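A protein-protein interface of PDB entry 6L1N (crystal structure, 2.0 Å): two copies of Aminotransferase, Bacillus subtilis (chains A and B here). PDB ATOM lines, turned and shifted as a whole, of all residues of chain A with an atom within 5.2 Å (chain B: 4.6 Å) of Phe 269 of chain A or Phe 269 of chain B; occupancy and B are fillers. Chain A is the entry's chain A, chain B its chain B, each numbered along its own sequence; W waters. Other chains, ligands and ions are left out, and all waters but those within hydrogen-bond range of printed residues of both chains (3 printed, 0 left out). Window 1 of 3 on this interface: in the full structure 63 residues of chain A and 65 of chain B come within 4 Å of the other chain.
Water W3 lies within hydrogen-bond range of O of Lys 104 of chain B (2.7 Å) and O of His 267 of chain A (2.8 Å). Water W2 lies within hydrogen-bond range of the backbone carbonyl oxygen of Val 268 of chain A (2.8 Å) and the backbone NH of Ala 105 of chain B (3.2 Å). Water W1 lies within hydrogen-bond range of the backbone carbonyl oxygen of Gly 271 of chain B (2.8 Å), the backbone NH of Val 270 of chain B (3.2 Å) and the backbone carbonyl oxygen of Gly 101 of chain A (3.5 Å).
Ala 105 of chain A touches Val 268 of chain B, and with the chains exchanged Val 268 of chain A touches Ala 105 of chain B. Ala 105 of chain A touches Phe 269 of chain B, but with the chains exchanged Phe 269 of chain A does not touch Ala 105 of chain B (4.03 Å). Phe 269 of chain A touches its own counterpart, Phe 269 of chain B. Positions printed for both chains: 69, 105, 109, 265, 267, 268, 269, 270 and 271. Of the 10 pairs that touch across the chains among the printed residues, 3 have their exchanged pair printed and touching as well.
CE1 of Phe 69 of chain A touches NZ of Lys 104 of chain B, 3.4 Å away. CB of Ala 105 of chain A touches CE1 of Phe 269 of chain B, at 3.98 Å. His 267 of chain A touches Lys 104 of chain B. Lys 104 of chain B touches Val 268 of chain A (C to O, 3.5 Å). CZ of Phe 269 of chain A touches CE1 of Phe 269 of chain B, at 3.9 Å. Val 270 of chain A touches Lys 104 of chain B.
Printed residues of chain B within 4 Å of Ala 105 of chain A: Val 268 and Phe 269. Of the printed residues of chain A, Lys 104 of chain B touches Phe 69 (3.4 Å), Asp 266 (2.6 Å), His 267 (3.5 Å), Val 268 (3.5 Å), Phe 269 (3.1 Å) and Val 270 (3.9 Å). Gln 265 of chain A touches none of the printed residues of chain B. The nearest residue of chain B that does not touch Phe 269 of chain A is Ala 105 of chain B (4.03 Å).
The backbone carbonyl oxygen of Val 268 of chain A sits at hydrogen-bond distance from the backbone NH of Ala 105 of chain B (3.2 Å). The backbone NH of Ala 105 of chain A sits at hydrogen-bond distance from the backbone carbonyl oxygen of Val 268 of chain B, 3.4 Å away. The backbone carbonyl oxygen (O) of Asp 266 of chain A lies within hydrogen-bond range of the side-chain amino group (NZ) of Lys 104 of chain B (2.6 Å). O of Phe 269 of chain A lies within hydrogen-bond range of NZ of Lys 104 of chain B.
Hydrophobic or aromatic side chains of chain A within 4 Å of the printed part of chain B: Phe 69, Ala 105, Phe 269 and Val 270. Of the 11 printed residues of chain B, 4 touch a printed residue of chain A. Along chain B the printed residues that touch a printed residue of chain A span positions 104 to 269.
The backbone carbonyl oxygen of Phe 69 of chain A sits at hydrogen-bond distance from the backbone NH of Gly 271 of chain A, 3.1 Å away.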
ATOM      1  N   PHE A  69      14.131   5.320 -27.500  1.00  0.00           N
ATOM      2  CA  PHE A  69      14.435   4.848 -26.131  1.00  0.00           C
ATOM      3  C   PHE A  69      14.938   3.422 -26.122  1.00  0.00           C
ATOM      4  O   PHE A  69      15.818   3.041 -25.320  1.00  0.00           O
ATOM      5  CB  PHE A  69      13.172   4.966 -25.244  1.00  0.00           C
ATOM      6  CG  PHE A  69      12.886   6.366 -24.828  1.00  0.00           C
ATOM      7  CD1 PHE A  69      13.429   6.863 -23.650  1.00  0.00           C
ATOM      8  CD2 PHE A  69      12.127   7.221 -25.643  1.00  0.00           C
ATOM      9  CE1 PHE A  69      13.194   8.187 -23.256  1.00  0.00           C
ATOM     10  CE2 PHE A  69      11.888   8.542 -25.238  1.00  0.00           C
ATOM     11  CZ  PHE A  69      12.438   9.023 -24.049  1.00  0.00           C
ATOM     12  N   GLY A 101      23.967  -1.368 -21.847  1.00  0.00           N
ATOM     13  CA  GLY A 101      25.288  -0.820 -21.757  1.00  0.00           C
ATOM     14  C   GLY A 101      26.280  -1.800 -21.183  1.00  0.00           C
ATOM     15  O   GLY A 101      26.903  -1.508 -20.169  1.00  0.00           O
ATOM     16  N   ALA A 105      25.476  -4.521 -16.981  1.00  0.00           N
ATOM     17  CA  ALA A 105      24.289  -3.677 -16.898  1.00  0.00           C
ATOM     18  C   ALA A 105      23.008  -4.500 -17.197  1.00  0.00           C
ATOM     19  O   ALA A 105      22.040  -4.381 -16.460  1.00  0.00           O
ATOM     20  CB  ALA A 105      24.411  -2.469 -17.825  1.00  0.00           C
ATOM     21  N   VAL A 109      19.719  -5.152 -14.664  1.00  0.00           N
ATOM     22  CA  VAL A 109      18.364  -4.773 -15.109  1.00  0.00           C
ATOM     23  C   VAL A 109      17.410  -5.981 -15.173  1.00  0.00           C
ATOM     24  O   VAL A 109      16.278  -5.920 -14.702  1.00  0.00           O
ATOM     25  CB  VAL A 109      18.423  -4.053 -16.483  1.00  0.00           C
ATOM     26  CG1 VAL A 109      17.030  -3.776 -17.032  1.00  0.00           C
ATOM     27  CG2 VAL A 109      19.186  -2.746 -16.376  1.00  0.00           C
ATOM     28  N   GLN A 265      14.054   0.423 -18.393  1.00  0.00           N
ATOM     29  CA  GLN A 265      15.046   1.235 -19.047  1.00  0.00           C
ATOM     30  C   GLN A 265      14.577   2.574 -19.571  1.00  0.00           C
ATOM     31  O   GLN A 265      15.360   3.539 -19.643  1.00  0.00           O
ATOM     32  CB  GLN A 265      15.707   0.428 -20.157  1.00  0.00           C
ATOM     33  CG  GLN A 265      16.444  -0.766 -19.567  1.00  0.00           C
ATOM     34  CD  GLN A 265      17.613  -1.248 -20.374  1.00  0.00           C
ATOM     35  OE1 GLN A 265      18.755  -1.313 -19.855  1.00  0.00           O
ATOM     36  NE2 GLN A 265      17.359  -1.611 -21.639  1.00  0.00           N
ATOM     37  N   ASP A 266      13.314   2.663 -19.911  1.00  0.00           N
ATOM     38  CA  ASP A 266      12.699   3.946 -20.275  1.00  0.00           C
ATOM     39  C   ASP A 266      12.912   5.043 -19.240  1.00  0.00           C
ATOM     40  O   ASP A 266      12.907   6.203 -19.609  1.00  0.00           O
ATOM     41  CB  ASP A 266      11.159   3.781 -20.455  1.00  0.00           C
ATOM     42  CG  ASP A 266      10.765   3.213 -21.833  1.00  0.00           C
ATOM     43  OD1 ASP A 266      11.646   2.971 -22.689  1.00  0.00           O
ATOM     44  OD2 ASP A 266       9.553   2.976 -22.037  1.00  0.00           O
ATOM     45  N   HIS A 267      13.063   4.675 -17.959  1.00  0.00           N
ATOM     46  CA  HIS A 267      13.288   5.629 -16.889  1.00  0.00           C
ATOM     47  C   HIS A 267      14.730   5.880 -16.514  1.00  0.00           C
ATOM     48  O   HIS A 267      14.982   6.741 -15.696  1.00  0.00           O
ATOM     49  CB  HIS A 267      12.559   5.196 -15.610  1.00  0.00           C
ATOM     50  CG  HIS A 267      11.077   5.127 -15.773  1.00  0.00           C
ATOM     51  ND1 HIS A 267      10.258   6.212 -15.570  1.00  0.00           N
ATOM     52  CD2 HIS A 267      10.273   4.112 -16.151  1.00  0.00           C
ATOM     53  CE1 HIS A 267       9.001   5.855 -15.774  1.00  0.00           C
ATOM     54  NE2 HIS A 267       8.994   4.593 -16.168  1.00  0.00           N
ATOM     55  N   VAL A 268      15.649   5.078 -17.044  1.00  0.00           N
ATOM     56  CA  VAL A 268      17.056   5.108 -16.638  1.00  0.00           C
ATOM     57  C   VAL A 268      17.991   5.514 -17.786  1.00  0.00           C
ATOM     58  O   VAL A 268      19.040   6.124 -17.564  1.00  0.00           O
ATOM     59  CB  VAL A 268      17.499   3.755 -16.079  1.00  0.00           C
ATOM     60  CG1 VAL A 268      18.942   3.814 -15.548  1.00  0.00           C
ATOM     61  CG2 VAL A 268      16.604   3.309 -14.970  1.00  0.00           C
ATOM     62  N   PHE A 269      17.583   5.176 -19.006  1.00  0.00           N
ATOM     63  CA  PHE A 269      18.321   5.400 -20.205  1.00  0.00           C
ATOM     64  C   PHE A 269      17.515   6.063 -21.301  1.00  0.00           C
ATOM     65  O   PHE A 269      16.266   6.078 -21.264  1.00  0.00           O
ATOM     66  CB  PHE A 269      18.790   4.052 -20.672  1.00  0.00           C
ATOM     67  CG  PHE A 269      19.648   3.340 -19.644  1.00  0.00           C
ATOM     68  CD1 PHE A 269      20.871   3.868 -19.269  1.00  0.00           C
ATOM     69  CD2 PHE A 269      19.222   2.149 -19.064  1.00  0.00           C
ATOM     70  CE1 PHE A 269      21.672   3.213 -18.325  1.00  0.00           C
ATOM     71  CE2 PHE A 269      19.994   1.510 -18.122  1.00  0.00           C
ATOM     72  CZ  PHE A 269      21.224   2.054 -17.747  1.00  0.00           C
ATOM     73  N   VAL A 270      18.243   6.586 -22.296  1.00  0.00           N
ATOM     74  CA  VAL A 270      17.635   6.927 -23.582  1.00  0.00           C
ATOM     75  C   VAL A 270      18.424   6.190 -24.662  1.00  0.00           C
ATOM     76  O   VAL A 270      19.239   6.807 -25.368  1.00  0.00           O
ATOM     77  CB  VAL A 270      17.661   8.452 -23.867  1.00  0.00           C
ATOM     78  CG1 VAL A 270      16.833   8.764 -25.132  1.00  0.00           C
ATOM     79  CG2 VAL A 270      17.089   9.276 -22.741  1.00  0.00           C
ATOM     80  N   GLY A 271      18.245   4.886 -24.739  1.00  0.00           N
ATOM     81  CA  GLY A 271      19.018   4.044 -25.655  1.00  0.00           C
ATOM     82  C   GLY A 271      20.489   4.133 -25.339  1.00  0.00           C
ATOM     83  O   GLY A 271      20.861   4.013 -24.167  1.00  0.00           O
ATOM     84  N   PHE B  69      37.478   1.201 -13.821  1.00  0.00           N
ATOM     85  CA  PHE B  69      36.035   1.049 -13.564  1.00  0.00           C
ATOM     86  C   PHE B  69      35.381   2.389 -13.261  1.00  0.00           C
ATOM     87  O   PHE B  69      34.241   2.641 -13.614  1.00  0.00           O
ATOM     88  CB  PHE B  69      35.807   0.120 -12.335  1.00  0.00           C
ATOM     89  CG  PHE B  69      36.141  -1.318 -12.580  1.00  0.00           C
ATOM     90  CD1 PHE B  69      35.127  -2.250 -12.842  1.00  0.00           C
ATOM     91  CD2 PHE B  69      37.478  -1.773 -12.521  1.00  0.00           C
ATOM     92  CE1 PHE B  69      35.441  -3.594 -13.063  1.00  0.00           C
ATOM     93  CE2 PHE B  69      37.788  -3.114 -12.748  1.00  0.00           C
ATOM     94  CZ  PHE B  69      36.766  -4.022 -13.029  1.00  0.00           C
ATOM     95  N   LYS B 104      20.144  10.971 -16.627  1.00  0.00           N
ATOM     96  CA  LYS B 104      19.056  10.070 -16.254  1.00  0.00           C
ATOM     97  C   LYS B 104      19.612   8.859 -15.458  1.00  0.00           C
ATOM     98  O   LYS B 104      19.023   8.427 -14.471  1.00  0.00           O
ATOM     99  CB  LYS B 104      18.349   9.603 -17.526  1.00  0.00           C
ATOM    100  CG  LYS B 104      16.872   9.548 -17.458  1.00  0.00           C
ATOM    101  CD  LYS B 104      16.269   9.387 -18.866  1.00  0.00           C
ATOM    102  CE  LYS B 104      15.019   8.572 -18.752  1.00  0.00           C
ATOM    103  NZ  LYS B 104      14.465   8.267 -20.051  1.00  0.00           N
ATOM    104  N   ALA B 105      20.724   8.299 -15.903  1.00  0.00           N
ATOM    105  CA  ALA B 105      21.329   7.196 -15.231  1.00  0.00           C
ATOM    106  C   ALA B 105      21.953   7.617 -13.896  1.00  0.00           C
ATOM    107  O   ALA B 105      21.829   6.911 -12.896  1.00  0.00           O
ATOM    108  CB  ALA B 105      22.365   6.512 -16.123  1.00  0.00           C
ATOM    109  N   VAL B 109      21.241   6.095 -10.097  1.00  0.00           N
ATOM    110  CA  VAL B 109      22.315   5.551  -9.302  1.00  0.00           C
ATOM    111  C   VAL B 109      22.334   6.289  -7.952  1.00  0.00           C
ATOM    112  O   VAL B 109      22.386   5.654  -6.891  1.00  0.00           O
ATOM    113  CB  VAL B 109      23.658   5.671 -10.027  1.00  0.00           C
ATOM    114  CG1 VAL B 109      24.824   5.256  -9.131  1.00  0.00           C
ATOM    115  CG2 VAL B 109      23.677   4.777 -11.264  1.00  0.00           C
ATOM    116  N   PHE B 264      28.628   1.140  -5.962  1.00  0.00           N
ATOM    117  CA  PHE B 264      27.548   0.661  -6.788  1.00  0.00           C
ATOM    118  C   PHE B 264      27.974   0.368  -8.221  1.00  0.00           C
ATOM    119  O   PHE B 264      27.748  -0.726  -8.687  1.00  0.00           O
ATOM    120  CB  PHE B 264      26.395   1.657  -6.808  1.00  0.00           C
ATOM    121  CG  PHE B 264      25.188   1.194  -7.599  1.00  0.00           C
ATOM    122  CD1 PHE B 264      24.193   0.415  -6.992  1.00  0.00           C
ATOM    123  CD2 PHE B 264      25.060   1.495  -8.946  1.00  0.00           C
ATOM    124  CE1 PHE B 264      23.072  -0.032  -7.737  1.00  0.00           C
ATOM    125  CE2 PHE B 264      23.946   1.087  -9.685  1.00  0.00           C
ATOM    126  CZ  PHE B 264      22.938   0.308  -9.078  1.00  0.00           C
ATOM    127  N   GLN B 265      28.493   1.385  -8.918  1.00  0.00           N
ATOM    128  CA  GLN B 265      28.785   1.326 -10.327  1.00  0.00           C
ATOM    129  C   GLN B 265      29.832   0.336 -10.744  1.00  0.00           C
ATOM    130  O   GLN B 265      29.786  -0.125 -11.913  1.00  0.00           O
ATOM    131  CB  GLN B 265      29.185   2.696 -10.877  1.00  0.00           C
ATOM    132  CG  GLN B 265      28.053   3.676 -10.770  1.00  0.00           C
ATOM    133  CD  GLN B 265      28.151   4.794 -11.790  1.00  0.00           C
ATOM    134  OE1 GLN B 265      27.260   4.930 -12.618  1.00  0.00           O
ATOM    135  NE2 GLN B 265      29.249   5.580 -11.743  1.00  0.00           N
ATOM    136  N   HIS B 267      29.902  -2.604  -9.947  1.00  0.00           N
ATOM    137  CA  HIS B 267      29.183  -3.854 -10.214  1.00  0.00           C
ATOM    138  C   HIS B 267      28.188  -3.778 -11.351  1.00  0.00           C
ATOM    139  O   HIS B 267      27.660  -4.817 -11.735  1.00  0.00           O
ATOM    140  CB  HIS B 267      28.436  -4.281  -8.966  1.00  0.00           C
ATOM    141  CG  HIS B 267      29.324  -4.606  -7.824  1.00  0.00           C
ATOM    142  ND1 HIS B 267      29.863  -5.858  -7.628  1.00  0.00           N
ATOM    143  CD2 HIS B 267      29.758  -3.848  -6.797  1.00  0.00           C
ATOM    144  CE1 HIS B 267      30.612  -5.849  -6.545  1.00  0.00           C
ATOM    145  NE2 HIS B 267      30.554  -4.643  -6.010  1.00  0.00           N
ATOM    146  N   VAL B 268      27.909  -2.580 -11.865  1.00  0.00           N
ATOM    147  CA  VAL B 268      26.833  -2.376 -12.852  1.00  0.00           C
ATOM    148  C   VAL B 268      27.301  -1.631 -14.113  1.00  0.00           C
ATOM    149  O   VAL B 268      26.926  -2.004 -15.208  1.00  0.00           O
ATOM    150  CB  VAL B 268      25.631  -1.653 -12.224  1.00  0.00           C
ATOM    151  CG1 VAL B 268      24.408  -1.660 -13.151  1.00  0.00           C
ATOM    152  CG2 VAL B 268      25.236  -2.296 -10.928  1.00  0.00           C
ATOM    153  N   PHE B 269      28.106  -0.574 -13.954  1.00  0.00           N
ATOM    154  CA  PHE B 269      28.688   0.238 -15.071  1.00  0.00           C
ATOM    155  C   PHE B 269      30.212   0.406 -15.064  1.00  0.00           C
ATOM    156  O   PHE B 269      30.695   1.241 -14.350  1.00  0.00           O
ATOM    157  CB  PHE B 269      28.106   1.609 -14.933  1.00  0.00           C
ATOM    158  CG  PHE B 269      26.624   1.618 -14.932  1.00  0.00           C
ATOM    159  CD1 PHE B 269      25.917   1.101 -16.020  1.00  0.00           C
ATOM    160  CD2 PHE B 269      25.930   2.107 -13.886  1.00  0.00           C
ATOM    161  CE1 PHE B 269      24.536   1.082 -16.022  1.00  0.00           C
ATOM    162  CE2 PHE B 269      24.532   2.110 -13.871  1.00  0.00           C
ATOM    163  CZ  PHE B 269      23.838   1.601 -14.943  1.00  0.00           C
ATOM    164  N   VAL B 270      30.976  -0.346 -15.847  1.00  0.00           N
ATOM    165  CA  VAL B 270      32.457  -0.324 -15.779  1.00  0.00           C
ATOM    166  C   VAL B 270      33.134   0.989 -16.304  1.00  0.00           C
ATOM    167  O   VAL B 270      34.294   0.981 -16.809  1.00  0.00           O
ATOM    168  CB  VAL B 270      33.012  -1.548 -16.553  1.00  0.00           C
ATOM    169  CG1 VAL B 270      33.037  -1.272 -18.017  1.00  0.00           C
ATOM    170  CG2 VAL B 270      34.420  -1.962 -16.119  1.00  0.00           C
ATOM    171  N   GLY B 271      32.460   2.129 -16.164  1.00  0.00           N
ATOM    172  CA  GLY B 271      32.912   3.321 -16.863  1.00  0.00           C
ATOM    173  C   GLY B 271      32.159   3.246 -18.174  1.00  0.00           C
ATOM    174  O   GLY B 271      31.130   2.498 -18.253  1.00  0.00           O
HETATM  175  O   HOH W   1      29.284   0.372 -18.433  1.00  0.00           O
HETATM  176  O   HOH W   2      20.935   7.634 -19.004  1.00  0.00           O
HETATM  177  O   HOH W   3      16.414   8.250 -13.820  1.00  0.00           O
